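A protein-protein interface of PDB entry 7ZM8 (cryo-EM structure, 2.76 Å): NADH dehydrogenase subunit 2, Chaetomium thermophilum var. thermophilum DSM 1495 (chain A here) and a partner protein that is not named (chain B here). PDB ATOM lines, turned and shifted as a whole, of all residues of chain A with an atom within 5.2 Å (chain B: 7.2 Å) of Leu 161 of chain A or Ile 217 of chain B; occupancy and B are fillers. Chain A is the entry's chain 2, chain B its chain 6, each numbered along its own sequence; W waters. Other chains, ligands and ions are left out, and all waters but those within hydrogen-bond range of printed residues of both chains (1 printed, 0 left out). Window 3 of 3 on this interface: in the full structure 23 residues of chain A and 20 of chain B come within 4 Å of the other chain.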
ATOM      1  N   ILE A 128     -21.923 -15.641  14.811  1.00  0.00           N
ATOM      2  CA  ILE A 128     -22.698 -14.744  13.962  1.00  0.00           C
ATOM      3  C   ILE A 128     -21.927 -14.374  12.702  1.00  0.00           C
ATOM      4  O   ILE A 128     -22.531 -14.157  11.648  1.00  0.00           O
ATOM      5  CB  ILE A 128     -23.137 -13.512  14.772  1.00  0.00           C
ATOM      6  CG1 ILE A 128     -23.998 -13.963  15.949  1.00  0.00           C
ATOM      7  CG2 ILE A 128     -23.936 -12.553  13.914  1.00  0.00           C
ATOM      8  CD1 ILE A 128     -24.746 -12.855  16.630  1.00  0.00           C
ATOM      9  N   TYR A 157     -29.220  -9.443   7.716  1.00  0.00           N
ATOM     10  CA  TYR A 157     -29.711  -9.569   9.107  1.00  0.00           C
ATOM     11  C   TYR A 157     -28.570  -9.869  10.073  1.00  0.00           C
ATOM     12  O   TYR A 157     -28.660  -9.460  11.228  1.00  0.00           O
ATOM     13  CB  TYR A 157     -30.869 -10.567   9.217  1.00  0.00           C
ATOM     14  CG  TYR A 157     -32.135 -10.210   8.486  1.00  0.00           C
ATOM     15  CD1 TYR A 157     -32.443  -8.900   8.172  1.00  0.00           C
ATOM     16  CD2 TYR A 157     -33.036 -11.194   8.121  1.00  0.00           C
ATOM     17  CE1 TYR A 157     -33.608  -8.577   7.501  1.00  0.00           C
ATOM     18  CE2 TYR A 157     -34.209 -10.890   7.454  1.00  0.00           C
ATOM     19  CZ  TYR A 157     -34.496  -9.575   7.144  1.00  0.00           C
ATOM     20  OH  TYR A 157     -35.644  -9.263   6.484  1.00  0.00           O
ATOM     21  N   GLY A 158     -27.544 -10.562   9.608  1.00  0.00           N
ATOM     22  CA  GLY A 158     -26.423 -10.910  10.489  1.00  0.00           C
ATOM     23  C   GLY A 158     -25.498  -9.727  10.621  1.00  0.00           C
ATOM     24  O   GLY A 158     -24.910  -9.585  11.689  1.00  0.00           O
ATOM     25  N   LEU A 159     -25.368  -8.916   9.578  1.00  0.00           N
ATOM     26  CA  LEU A 159     -24.614  -7.672   9.654  1.00  0.00           C
ATOM     27  C   LEU A 159     -25.262  -6.686  10.619  1.00  0.00           C
ATOM     28  O   LEU A 159     -24.560  -5.956  11.324  1.00  0.00           O
ATOM     29  CB  LEU A 159     -24.468  -7.067   8.263  1.00  0.00           C
ATOM     30  CG  LEU A 159     -23.416  -7.772   7.403  1.00  0.00           C
ATOM     31  CD1 LEU A 159     -23.493  -7.337   5.957  1.00  0.00           C
ATOM     32  CD2 LEU A 159     -22.031  -7.540   7.958  1.00  0.00           C
ATOM     33  N   TYR A 160     -26.598  -6.651  10.667  1.00  0.00           N
ATOM     34  CA  TYR A 160     -27.281  -5.794  11.634  1.00  0.00           C
ATOM     35  C   TYR A 160     -26.982  -6.233  13.057  1.00  0.00           C
ATOM     36  O   TYR A 160     -26.782  -5.400  13.944  1.00  0.00           O
ATOM     37  CB  TYR A 160     -28.793  -5.805  11.405  1.00  0.00           C
ATOM     38  CG  TYR A 160     -29.243  -5.440  10.015  1.00  0.00           C
ATOM     39  CD1 TYR A 160     -28.455  -4.655   9.189  1.00  0.00           C
ATOM     40  CD2 TYR A 160     -30.460  -5.886   9.529  1.00  0.00           C
ATOM     41  CE1 TYR A 160     -28.863  -4.334   7.923  1.00  0.00           C
ATOM     42  CE2 TYR A 160     -30.876  -5.566   8.267  1.00  0.00           C
ATOM     43  CZ  TYR A 160     -30.072  -4.790   7.470  1.00  0.00           C
ATOM     44  OH  TYR A 160     -30.483  -4.474   6.207  1.00  0.00           O
ATOM     45  N   LEU A 161     -26.962  -7.542  13.292  1.00  0.00           N
ATOM     46  CA  LEU A 161     -26.717  -8.071  14.625  1.00  0.00           C
ATOM     47  C   LEU A 161     -25.275  -7.867  15.056  1.00  0.00           C
ATOM     48  O   LEU A 161     -25.003  -7.707  16.249  1.00  0.00           O
ATOM     49  CB  LEU A 161     -27.071  -9.551  14.656  1.00  0.00           C
ATOM     50  CG  LEU A 161     -28.559  -9.822  14.495  1.00  0.00           C
ATOM     51  CD1 LEU A 161     -28.788 -11.283  14.170  1.00  0.00           C
ATOM     52  CD2 LEU A 161     -29.301  -9.408  15.752  1.00  0.00           C
ATOM     53  N   LEU A 162     -24.340  -7.906  14.109  1.00  0.00           N
ATOM     54  CA  LEU A 162     -22.950  -7.600  14.415  1.00  0.00           C
ATOM     55  C   LEU A 162     -22.797  -6.163  14.874  1.00  0.00           C
ATOM     56  O   LEU A 162     -22.042  -5.874  15.806  1.00  0.00           O
ATOM     57  CB  LEU A 162     -22.091  -7.849  13.185  1.00  0.00           C
ATOM     58  CG  LEU A 162     -21.802  -9.291  12.827  1.00  0.00           C
ATOM     59  CD1 LEU A 162     -20.708  -9.301  11.804  1.00  0.00           C
ATOM     60  CD2 LEU A 162     -21.369 -10.042  14.075  1.00  0.00           C
ATOM     61  N   SER A 163     -23.508  -5.248  14.225  1.00  0.00           N
ATOM     62  CA  SER A 163     -23.395  -3.839  14.551  1.00  0.00           C
ATOM     63  C   SER A 163     -23.996  -3.510  15.906  1.00  0.00           C
ATOM     64  O   SER A 163     -23.635  -2.489  16.495  1.00  0.00           O
ATOM     65  CB  SER A 163     -24.065  -3.013  13.459  1.00  0.00           C
ATOM     66  OG  SER A 163     -23.469  -3.273  12.204  1.00  0.00           O
ATOM     67  N   THR A 164     -24.895  -4.345  16.412  1.00  0.00           N
ATOM     68  CA  THR A 164     -25.580  -4.101  17.671  1.00  0.00           C
ATOM     69  C   THR A 164     -25.047  -4.972  18.803  1.00  0.00           C
ATOM     70  O   THR A 164     -25.481  -4.815  19.947  1.00  0.00           O
ATOM     71  CB  THR A 164     -27.085  -4.332  17.471  1.00  0.00           C
ATOM     72  OG1 THR A 164     -27.499  -3.662  16.278  1.00  0.00           O
ATOM     73  CG2 THR A 164     -27.903  -3.759  18.618  1.00  0.00           C
ATOM     74  N   ILE A 165     -24.065  -5.831  18.510  1.00  0.00           N
ATOM     75  CA  ILE A 165     -23.575  -6.844  19.497  1.00  0.00           C
ATOM     76  C   ILE A 165     -22.895  -6.217  20.720  1.00  0.00           C
ATOM     77  O   ILE A 165     -22.956  -6.834  21.798  1.00  0.00           O
ATOM     78  CB  ILE A 165     -22.762  -7.963  18.805  1.00  0.00           C
ATOM     79  CG1 ILE A 165     -22.967  -9.319  19.486  1.00  0.00           C
ATOM     80  CG2 ILE A 165     -21.293  -7.605  18.657  1.00  0.00           C
ATOM     81  CD1 ILE A 165     -22.566 -10.501  18.638  1.00  0.00           C
ATOM     82  N   ARG A 167     -23.688  -4.348  23.263  1.00  0.00           N
ATOM     83  CA  ARG A 167     -24.981  -3.822  23.776  1.00  0.00           C
ATOM     84  C   ARG A 167     -24.777  -2.682  24.769  1.00  0.00           C
ATOM     85  O   ARG A 167     -25.730  -1.922  24.969  1.00  0.00           O
ATOM     86  CB  ARG A 167     -25.815  -4.975  24.341  1.00  0.00           C
ATOM     87  CG  ARG A 167     -25.098  -5.854  25.354  1.00  0.00           C
ATOM     88  CD  ARG A 167     -25.934  -7.062  25.733  1.00  0.00           C
ATOM     89  NE  ARG A 167     -27.250  -6.721  26.252  1.00  0.00           N
ATOM     90  CZ  ARG A 167     -27.537  -6.548  27.537  1.00  0.00           C
ATOM     91  NH1 ARG A 167     -28.769  -6.240  27.902  1.00  0.00           N
ATOM     92  NH2 ARG A 167     -26.598  -6.685  28.455  1.00  0.00           N
ATOM     93  N   LEU B 209     -31.064 -17.535  12.922  1.00  0.00           N
ATOM     94  CA  LEU B 209     -30.314 -16.312  13.177  1.00  0.00           C
ATOM     95  C   LEU B 209     -31.148 -15.297  13.953  1.00  0.00           C
ATOM     96  O   LEU B 209     -30.634 -14.620  14.847  1.00  0.00           O
ATOM     97  CB  LEU B 209     -29.835 -15.716  11.857  1.00  0.00           C
ATOM     98  CG  LEU B 209     -29.060 -14.402  11.916  1.00  0.00           C
ATOM     99  CD1 LEU B 209     -27.701 -14.622  12.525  1.00  0.00           C
ATOM    100  CD2 LEU B 209     -28.934 -13.807  10.531  1.00  0.00           C
ATOM    101  N   ALA B 210     -32.430 -15.170  13.617  1.00  0.00           N
ATOM    102  CA  ALA B 210     -33.288 -14.237  14.330  1.00  0.00           C
ATOM    103  C   ALA B 210     -33.519 -14.669  15.768  1.00  0.00           C
ATOM    104  O   ALA B 210     -33.893 -13.846  16.609  1.00  0.00           O
ATOM    105  CB  ALA B 210     -34.617 -14.084  13.595  1.00  0.00           C
ATOM    106  N   MET B 211     -33.315 -15.950  16.070  1.00  0.00           N
ATOM    107  CA  MET B 211     -33.432 -16.426  17.441  1.00  0.00           C
ATOM    108  C   MET B 211     -32.184 -16.101  18.245  1.00  0.00           C
ATOM    109  O   MET B 211     -32.259 -15.441  19.284  1.00  0.00           O
ATOM    110  CB  MET B 211     -33.686 -17.930  17.450  1.00  0.00           C
ATOM    111  CG  MET B 211     -33.638 -18.558  18.827  1.00  0.00           C
ATOM    112  SD  MET B 211     -35.127 -18.233  19.780  1.00  0.00           S
ATOM    113  CE  MET B 211     -36.257 -19.387  19.013  1.00  0.00           C
ATOM    114  N   VAL B 212     -31.029 -16.563  17.772  1.00  0.00           N
ATOM    115  CA  VAL B 212     -29.780 -16.352  18.490  1.00  0.00           C
ATOM    116  C   VAL B 212     -29.438 -14.871  18.557  1.00  0.00           C
ATOM    117  O   VAL B 212     -29.043 -14.358  19.609  1.00  0.00           O
ATOM    118  CB  VAL B 212     -28.659 -17.164  17.820  1.00  0.00           C
ATOM    119  CG1 VAL B 212     -27.302 -16.760  18.363  1.00  0.00           C
ATOM    120  CG2 VAL B 212     -28.904 -18.641  18.011  1.00  0.00           C
ATOM    121  N   GLY B 213     -29.585 -14.161  17.438  1.00  0.00           N
ATOM    122  CA  GLY B 213     -29.161 -12.775  17.393  1.00  0.00           C
ATOM    123  C   GLY B 213     -30.008 -11.854  18.248  1.00  0.00           C
ATOM    124  O   GLY B 213     -29.490 -10.931  18.876  1.00  0.00           O
ATOM    125  N   ALA B 214     -31.306 -12.118  18.324  1.00  0.00           N
ATOM    126  CA  ALA B 214     -32.193 -11.197  19.070  1.00  0.00           C
ATOM    127  C   ALA B 214     -31.957 -11.367  20.568  1.00  0.00           C
ATOM    128  O   ALA B 214     -31.925 -10.351  21.266  1.00  0.00           O
ATOM    129  CB  ALA B 214     -33.630 -11.380  18.662  1.00  0.00           C
ATOM    130  N   ILE B 215     -31.786 -12.605  21.021  1.00  0.00           N
ATOM    131  CA  ILE B 215     -31.475 -12.888  22.451  1.00  0.00           C
ATOM    132  C   ILE B 215     -30.115 -12.291  22.841  1.00  0.00           C
ATOM    133  O   ILE B 215     -30.047 -11.654  23.896  1.00  0.00           O
ATOM    134  CB  ILE B 215     -31.530 -14.410  22.680  1.00  0.00           C
ATOM    135  CG1 ILE B 215     -32.950 -14.957  22.516  1.00  0.00           C
ATOM    136  CG2 ILE B 215     -30.937 -14.790  24.024  1.00  0.00           C
ATOM    137  CD1 ILE B 215     -33.013 -16.463  22.426  1.00  0.00           C
ATOM    138  N   VAL B 216     -29.093 -12.429  21.992  1.00  0.00           N
ATOM    139  CA  VAL B 216     -27.716 -11.934  22.297  1.00  0.00           C
ATOM    140  C   VAL B 216     -27.708 -10.412  22.456  1.00  0.00           C
ATOM    141  O   VAL B 216     -26.956  -9.924  23.300  1.00  0.00           O
ATOM    142  CB  VAL B 216     -26.638 -12.470  21.336  1.00  0.00           C
ATOM    143  CG1 VAL B 216     -26.604 -11.733  20.010  1.00  0.00           C
ATOM    144  CG2 VAL B 216     -25.263 -12.457  21.976  1.00  0.00           C
ATOM    145  N   ILE B 217     -28.508  -9.690  21.679  1.00  0.00           N
ATOM    146  CA  ILE B 217     -28.487  -8.202  21.733  1.00  0.00           C
ATOM    147  C   ILE B 217     -29.350  -7.673  22.877  1.00  0.00           C
ATOM    148  O   ILE B 217     -29.118  -6.552  23.298  1.00  0.00           O
ATOM    149  CB  ILE B 217     -28.843  -7.583  20.368  1.00  0.00           C
ATOM    150  CG1 ILE B 217     -30.303  -7.836  19.987  1.00  0.00           C
ATOM    151  CG2 ILE B 217     -27.860  -8.034  19.298  1.00  0.00           C
ATOM    152  CD1 ILE B 217     -30.709  -7.241  18.669  1.00  0.00           C
ATOM    153  N   THR B 218     -30.295  -8.454  23.381  1.00  0.00           N
ATOM    154  CA  THR B 218     -31.224  -7.926  24.425  1.00  0.00           C
ATOM    155  C   THR B 218     -30.993  -8.423  25.859  1.00  0.00           C
ATOM    156  O   THR B 218     -31.060  -7.597  26.756  1.00  0.00           O
ATOM    157  CB  THR B 218     -32.693  -8.038  23.970  1.00  0.00           C
ATOM    158  OG1 THR B 218     -32.943  -9.401  23.627  1.00  0.00           O
ATOM    159  CG2 THR B 218     -33.047  -7.135  22.812  1.00  0.00           C
ATOM    160  N   ILE B 219     -30.774  -9.705  26.078  1.00  0.00           N
ATOM    161  CA  ILE B 219     -30.719 -10.269  27.462  1.00  0.00           C
ATOM    162  C   ILE B 219     -29.368 -10.083  28.141  1.00  0.00           C
ATOM    163  O   ILE B 219     -28.363  -9.957  27.446  1.00  0.00           O
ATOM    164  CB  ILE B 219     -31.202 -11.737  27.495  1.00  0.00           C
ATOM    165  CG1 ILE B 219     -30.073 -12.731  27.218  1.00  0.00           C
ATOM    166  CG2 ILE B 219     -32.390 -11.945  26.571  1.00  0.00           C
ATOM    167  CD1 ILE B 219     -30.344 -14.116  27.746  1.00  0.00           C
ATOM    168  N   LYS B 220     -29.377 -10.056  29.469  1.00  0.00           N
ATOM    169  CA  LYS B 220     -28.117  -9.980  30.228  1.00  0.00           C
ATOM    170  C   LYS B 220     -27.680 -11.422  30.417  1.00  0.00           C
ATOM    171  O   LYS B 220     -28.477 -12.209  30.942  1.00  0.00           O
ATOM    172  CB  LYS B 220     -28.364  -9.340  31.593  1.00  0.00           C
ATOM    173  CG  LYS B 220     -27.137  -9.141  32.472  1.00  0.00           C
ATOM    174  CD  LYS B 220     -26.190  -8.087  31.948  1.00  0.00           C
ATOM    175  CE  LYS B 220     -24.949  -7.938  32.799  1.00  0.00           C
ATOM    176  NZ  LYS B 220     -25.281  -7.547  34.189  1.00  0.00           N
HETATM  177  O   HOH W   1     -24.310  -9.113  22.838  1.00  0.00           O
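NE of Arg 167 of chain A is in hydrogen-bond range of O of Ile 217 of chain B (3.5 Å).
The guanidinium group (NH1) of Arg 167 of chain A sits at hydrogen-bond distance from the backbone carbonyl oxygen (O) of Thr 218 of chain B (2.9 Å).
The backbone carbonyl oxygen (O) of Ala 214 of chain B sits at hydrogen-bond distance from the side-chain hydroxyl (OG1) of Thr 218 of chain B, at 2.7 Å.
Leu 209 of chain B touches Tyr 157 of chain A (CD2 to C, 3.98 Å).
Leu 209 of chain B touches Gly 158 of chain A.
Leu 161 of chain A touches Leu 209 of chain B.
O of Gly 213 of chain B touches CD2 of Leu 161 of chain A (3.5 Å).
Ile 217 of chain B touches Leu 161 of chain A (CD1 to CD2, 3.9 Å).
CD of Arg 167 of chain A touches O of Val 216 of chain B (3.9 Å).
Ile 219 of chain B touches Arg 167 of chain A.
Arg 167 of chain A touches Lys 220 of chain B (NH2 to CD, 3.8 Å).
Ile 128 of chain A touches none of the printed residues of chain B.
Printed residues of chain B within 4 Å of Gly 158 of chain A: Leu 209.
Leu 161 of chain A touches just these residues of chain B: Leu 209 (3.9 Å), Gly 213 (3.5 Å) and Ile 217 (3.9 Å).
Printed residues of chain B within 4 Å of Arg 167 of chain A: Val 216, Ile 217, Thr 218, Ile 219 and Lys 220.
The nearest residue of chain B that does not touch Leu 161 of chain A is Ala 214 of chain B (4.2 Å).
The nearest printed residue of chain A that does not touch Leu 209 of chain B is Ile 128 of chain A (4.5 Å).
Printed residues of chain B that touch a printed residue of chain A: Leu 209, Gly 213, Val 216, Ile 217, Thr 218, Ile 219 and Lys 220.
Hydrophobic or aromatic side chains of chain B within 4 Å of the printed part of chain A: Leu 209 and Ile 217.
Along chain A the printed residues that touch a printed residue of chain B span positions 157 to 167.
Among the printed residues, 10 pairs touch across the chains.
Among the printed residues, no Asp or Glu carboxylate lies within 4 Å of a Lys or Arg side-chain nitrogen of the other chain.
Water W1 lies within hydrogen-bond range of the backbone carbonyl oxygen of Val 216 of chain B and the backbone carbonyl oxygen of Ile 165 of chain A.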
